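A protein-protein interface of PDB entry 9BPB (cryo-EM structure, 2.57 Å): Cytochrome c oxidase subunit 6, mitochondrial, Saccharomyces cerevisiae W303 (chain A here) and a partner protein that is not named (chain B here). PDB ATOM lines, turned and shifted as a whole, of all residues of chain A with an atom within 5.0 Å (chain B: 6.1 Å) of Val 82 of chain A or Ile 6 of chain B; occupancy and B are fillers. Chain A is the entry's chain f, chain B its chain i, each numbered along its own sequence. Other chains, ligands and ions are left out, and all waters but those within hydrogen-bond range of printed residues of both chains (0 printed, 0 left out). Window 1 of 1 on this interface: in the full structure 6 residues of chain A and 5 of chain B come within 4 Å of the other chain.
Thr 7 of chain B touches Phe 49 of chain A (CG2 to CE1, 3.5 Å).
CA of Gly 8 of chain B touches OD2 of Asp 80 of chain A, 3.98 Å away.
Leu 81 of chain A touches Ile 6 of chain B.
Leu 81 of chain A touches Thr 7 of chain B.
OE1 of Gln 120 of chain A touches CG1 of Ile 6 of chain B, 3.3 Å away.
Of the 7 printed residues of chain B, 3 touch a printed residue of chain A.
Printed residues of chain B that touch a printed residue of chain A: Ile 6, Thr 7 and Gly 8.
Printed residues of chain A that touch a printed residue of chain B: Phe 49, Asp 80, Leu 81, Val 82 and Gln 120.
Of the printed residues of chain B, Val 82 of chain A touches Ile 6.
Of chain A, only Leu 81 (3.8 Å), Val 82 (3.3 Å) and Gln 120 (3.3 Å) come within 4 Å of Ile 6 of chain B.
Of the printed residues of chain B, Asp 80 of chain A touches Gly 8 (3.98 Å).
Printed residues of chain B within 4 Å of Phe 49 of chain A: Thr 7.
Of the printed residues of chain B, Leu 81 of chain A touches Ile 6 (3.8 Å) and Thr 7 (3.9 Å).
Of the printed residues of chain A, Thr 7 of chain B touches Phe 49 (3.5 Å) and Leu 81 (3.9 Å).
Ile 3 of chain B touches none of the printed residues of chain A.
Pro 5 of chain B touches none of the printed residues of chain A.
The nearest residue of chain B that does not touch Val 82 of chain A is Thr 7 of chain B (5.3 Å).
N of Val 82 of chain A is in hydrogen-bond range of O of Ile 6 of chain B, 3.3 Å away.
The backbone carbonyl oxygen of Val 115 of chain A sits close to the side-chain amide oxygen of Gln 120 of chain A (3.4 Å).
The side-chain amide nitrogen of Asn 117 of chain A lies within hydrogen-bond range of the side-chain amide oxygen of Gln 120 of chain A.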
ATOM      1  N   PHE A  49      17.322  25.137  15.018  1.00  0.00           N
ATOM      2  CA  PHE A  49      16.989  23.771  15.406  1.00  0.00           C
ATOM      3  C   PHE A  49      15.485  23.584  15.556  1.00  0.00           C
ATOM      4  O   PHE A  49      14.929  22.579  15.096  1.00  0.00           O
ATOM      5  CB  PHE A  49      17.706  23.408  16.706  1.00  0.00           C
ATOM      6  CG  PHE A  49      18.030  21.949  16.833  1.00  0.00           C
ATOM      7  CD1 PHE A  49      19.139  21.415  16.197  1.00  0.00           C
ATOM      8  CD2 PHE A  49      17.233  21.113  17.594  1.00  0.00           C
ATOM      9  CE1 PHE A  49      19.443  20.073  16.311  1.00  0.00           C
ATOM     10  CE2 PHE A  49      17.532  19.770  17.715  1.00  0.00           C
ATOM     11  CZ  PHE A  49      18.638  19.250  17.072  1.00  0.00           C
ATOM     12  N   ASP A  80      23.914  17.825   9.443  1.00  0.00           N
ATOM     13  CA  ASP A  80      24.992  17.714  10.422  1.00  0.00           C
ATOM     14  C   ASP A  80      24.447  17.459  11.822  1.00  0.00           C
ATOM     15  O   ASP A  80      25.007  16.661  12.582  1.00  0.00           O
ATOM     16  CB  ASP A  80      25.841  18.983  10.390  1.00  0.00           C
ATOM     17  CG  ASP A  80      27.121  18.853  11.187  1.00  0.00           C
ATOM     18  OD1 ASP A  80      27.403  17.748  11.695  1.00  0.00           O
ATOM     19  OD2 ASP A  80      27.853  19.859  11.291  1.00  0.00           O
ATOM     20  N   LEU A  81      23.358  18.129  12.179  1.00  0.00           N
ATOM     21  CA  LEU A  81      22.760  17.959  13.494  1.00  0.00           C
ATOM     22  C   LEU A  81      22.134  16.574  13.638  1.00  0.00           C
ATOM     23  O   LEU A  81      21.578  16.021  12.686  1.00  0.00           O
ATOM     24  CB  LEU A  81      21.719  19.057  13.724  1.00  0.00           C
ATOM     25  CG  LEU A  81      20.497  19.163  12.796  1.00  0.00           C
ATOM     26  CD1 LEU A  81      19.377  18.220  13.210  1.00  0.00           C
ATOM     27  CD2 LEU A  81      19.988  20.596  12.702  1.00  0.00           C
ATOM     28  N   VAL A  82      22.257  16.000  14.827  1.00  0.00           N
ATOM     29  CA  VAL A  82      21.469  14.804  15.147  1.00  0.00           C
ATOM     30  C   VAL A  82      20.028  15.226  15.411  1.00  0.00           C
ATOM     31  O   VAL A  82      19.797  16.177  16.177  1.00  0.00           O
ATOM     32  CB  VAL A  82      22.062  14.077  16.356  1.00  0.00           C
ATOM     33  CG1 VAL A  82      21.231  12.850  16.701  1.00  0.00           C
ATOM     34  CG2 VAL A  82      23.501  13.682  16.077  1.00  0.00           C
ATOM     35  N   PRO A  83      19.037  14.576  14.801  1.00  0.00           N
ATOM     36  CA  PRO A  83      17.651  15.028  14.966  1.00  0.00           C
ATOM     37  C   PRO A  83      17.162  14.875  16.400  1.00  0.00           C
ATOM     38  O   PRO A  83      17.648  14.040  17.164  1.00  0.00           O
ATOM     39  CB  PRO A  83      16.867  14.121  14.010  1.00  0.00           C
ATOM     40  CG  PRO A  83      17.760  12.941  13.781  1.00  0.00           C
ATOM     41  CD  PRO A  83      19.145  13.493  13.812  1.00  0.00           C
ATOM     42  N   ALA A  84      16.190  15.710  16.757  1.00  0.00           N
ATOM     43  CA  ALA A  84      15.579  15.656  18.072  1.00  0.00           C
ATOM     44  C   ALA A  84      14.715  14.403  18.205  1.00  0.00           C
ATOM     45  O   ALA A  84      14.249  13.851  17.205  1.00  0.00           O
ATOM     46  CB  ALA A  84      14.736  16.905  18.311  1.00  0.00           C
ATOM     47  N   LYS A 114      24.602   7.790  14.218  1.00  0.00           N
ATOM     48  CA  LYS A 114      24.477   9.242  14.170  1.00  0.00           C
ATOM     49  C   LYS A 114      24.618   9.893  15.539  1.00  0.00           C
ATOM     50  O   LYS A 114      25.207  10.973  15.644  1.00  0.00           O
ATOM     51  CB  LYS A 114      23.131   9.631  13.558  1.00  0.00           C
ATOM     52  CG  LYS A 114      22.975  11.112  13.281  1.00  0.00           C
ATOM     53  CD  LYS A 114      23.914  11.584  12.192  1.00  0.00           C
ATOM     54  CE  LYS A 114      23.566  12.995  11.762  1.00  0.00           C
ATOM     55  NZ  LYS A 114      24.338  13.411  10.570  1.00  0.00           N
ATOM     56  N   VAL A 115      24.094   9.258  16.589  1.00  0.00           N
ATOM     57  CA  VAL A 115      24.010   9.922  17.885  1.00  0.00           C
ATOM     58  C   VAL A 115      25.398  10.163  18.468  1.00  0.00           C
ATOM     59  O   VAL A 115      25.600  11.122  19.221  1.00  0.00           O
ATOM     60  CB  VAL A 115      23.114   9.108  18.838  1.00  0.00           C
ATOM     61  CG1 VAL A 115      23.750   7.766  19.181  1.00  0.00           C
ATOM     62  CG2 VAL A 115      22.775   9.910  20.074  1.00  0.00           C
ATOM     63  N   ASN A 117      27.106   9.093  20.763  1.00  0.00           N
ATOM     64  CA  ASN A 117      27.335   8.899  22.189  1.00  0.00           C
ATOM     65  C   ASN A 117      26.627   7.641  22.666  1.00  0.00           C
ATOM     66  O   ASN A 117      25.509   7.342  22.236  1.00  0.00           O
ATOM     67  CB  ASN A 117      26.866  10.113  22.994  1.00  0.00           C
ATOM     68  CG  ASN A 117      27.861  11.251  22.952  1.00  0.00           C
ATOM     69  OD1 ASN A 117      29.041  11.069  23.253  1.00  0.00           O
ATOM     70  ND2 ASN A 117      27.400  12.431  22.553  1.00  0.00           N
ATOM     71  N   GLN A 120      23.768   8.911  25.022  1.00  0.00           N
ATOM     72  CA  GLN A 120      22.710   9.608  24.300  1.00  0.00           C
ATOM     73  C   GLN A 120      21.857   8.642  23.490  1.00  0.00           C
ATOM     74  O   GLN A 120      20.661   8.885  23.301  1.00  0.00           O
ATOM     75  CB  GLN A 120      23.309  10.684  23.399  1.00  0.00           C
ATOM     76  CG  GLN A 120      23.555  12.006  24.102  1.00  0.00           C
ATOM     77  CD  GLN A 120      24.540  12.881  23.359  1.00  0.00           C
ATOM     78  OE1 GLN A 120      24.911  12.591  22.222  1.00  0.00           O
ATOM     79  NE2 GLN A 120      24.979  13.957  24.002  1.00  0.00           N
ATOM     80  N   TYR A 124      17.875   8.586  23.866  1.00  0.00           N
ATOM     81  CA  TYR A 124      16.841   8.351  22.866  1.00  0.00           C
ATOM     82  C   TYR A 124      16.098   7.051  23.137  1.00  0.00           C
ATOM     83  O   TYR A 124      14.900   6.954  22.854  1.00  0.00           O
ATOM     84  CB  TYR A 124      17.443   8.314  21.462  1.00  0.00           C
ATOM     85  CG  TYR A 124      17.785   9.661  20.866  1.00  0.00           C
ATOM     86  CD1 TYR A 124      19.007  10.265  21.120  1.00  0.00           C
ATOM     87  CD2 TYR A 124      16.890  10.318  20.033  1.00  0.00           C
ATOM     88  CE1 TYR A 124      19.326  11.491  20.568  1.00  0.00           C
ATOM     89  CE2 TYR A 124      17.199  11.545  19.479  1.00  0.00           C
ATOM     90  CZ  TYR A 124      18.418  12.127  19.749  1.00  0.00           C
ATOM     91  OH  TYR A 124      18.731  13.346  19.200  1.00  0.00           O
ATOM     92  N   ILE B   3      17.077  16.635  26.674  1.00  0.00           N
ATOM     93  CA  ILE B   3      17.857  16.149  25.543  1.00  0.00           C
ATOM     94  C   ILE B   3      18.812  17.231  25.049  1.00  0.00           C
ATOM     95  O   ILE B   3      18.387  18.315  24.650  1.00  0.00           O
ATOM     96  CB  ILE B   3      16.943  15.669  24.405  1.00  0.00           C
ATOM     97  CG1 ILE B   3      16.205  14.395  24.815  1.00  0.00           C
ATOM     98  CG2 ILE B   3      17.749  15.437  23.138  1.00  0.00           C
ATOM     99  CD1 ILE B   3      17.097  13.175  24.915  1.00  0.00           C
ATOM    100  N   ALA B   4      20.101  16.926  25.081  1.00  0.00           N
ATOM    101  CA  ALA B   4      21.106  17.878  24.623  1.00  0.00           C
ATOM    102  C   ALA B   4      21.054  17.997  23.105  1.00  0.00           C
ATOM    103  O   ALA B   4      21.106  16.980  22.408  1.00  0.00           O
ATOM    104  CB  ALA B   4      22.498  17.444  25.072  1.00  0.00           C
ATOM    105  N   PRO B   5      20.939  19.202  22.558  1.00  0.00           N
ATOM    106  CA  PRO B   5      20.909  19.352  21.097  1.00  0.00           C
ATOM    107  C   PRO B   5      22.275  19.162  20.454  1.00  0.00           C
ATOM    108  O   PRO B   5      22.994  20.140  20.231  1.00  0.00           O
ATOM    109  CB  PRO B   5      20.400  20.787  20.900  1.00  0.00           C
ATOM    110  CG  PRO B   5      19.760  21.161  22.205  1.00  0.00           C
ATOM    111  CD  PRO B   5      20.540  20.436  23.251  1.00  0.00           C
ATOM    112  N   ILE B   6      22.648  17.916  20.165  1.00  0.00           N
ATOM    113  CA  ILE B   6      23.944  17.630  19.550  1.00  0.00           C
ATOM    114  C   ILE B   6      23.994  18.331  18.197  1.00  0.00           C
ATOM    115  O   ILE B   6      23.248  17.977  17.279  1.00  0.00           O
ATOM    116  CB  ILE B   6      24.190  16.124  19.393  1.00  0.00           C
ATOM    117  CG1 ILE B   6      24.118  15.392  20.733  1.00  0.00           C
ATOM    118  CG2 ILE B   6      25.540  15.874  18.737  1.00  0.00           C
ATOM    119  CD1 ILE B   6      22.761  14.803  21.037  1.00  0.00           C
ATOM    120  N   THR B   7      24.874  19.320  18.065  1.00  0.00           N
ATOM    121  CA  THR B   7      25.065  20.028  16.808  1.00  0.00           C
ATOM    122  C   THR B   7      26.547  20.306  16.614  1.00  0.00           C
ATOM    123  O   THR B   7      27.340  20.266  17.558  1.00  0.00           O
ATOM    124  CB  THR B   7      24.287  21.353  16.757  1.00  0.00           C
ATOM    125  OG1 THR B   7      24.683  22.188  17.851  1.00  0.00           O
ATOM    126  CG2 THR B   7      22.786  21.112  16.813  1.00  0.00           C
ATOM    127  N   GLY B   8      26.914  20.583  15.365  1.00  0.00           N
ATOM    128  CA  GLY B   8      28.257  21.034  15.068  1.00  0.00           C
ATOM    129  C   GLY B   8      29.350  20.021  15.316  1.00  0.00           C
ATOM    130  O   GLY B   8      30.509  20.407  15.491  1.00  0.00           O
ATOM    131  N   THR B   9      29.012  18.729  15.345  1.00  0.00           N
ATOM    132  CA  THR B   9      30.042  17.702  15.466  1.00  0.00           C
ATOM    133  C   THR B   9      31.079  17.844  14.361  1.00  0.00           C
ATOM    134  O   THR B   9      32.279  17.659  14.595  1.00  0.00           O
ATOM    135  CB  THR B   9      29.410  16.311  15.424  1.00  0.00           C
ATOM    136  OG1 THR B   9      28.390  16.214  16.423  1.00  0.00           O
ATOM    137  CG2 THR B   9      30.461  15.238  15.668  1.00  0.00           C
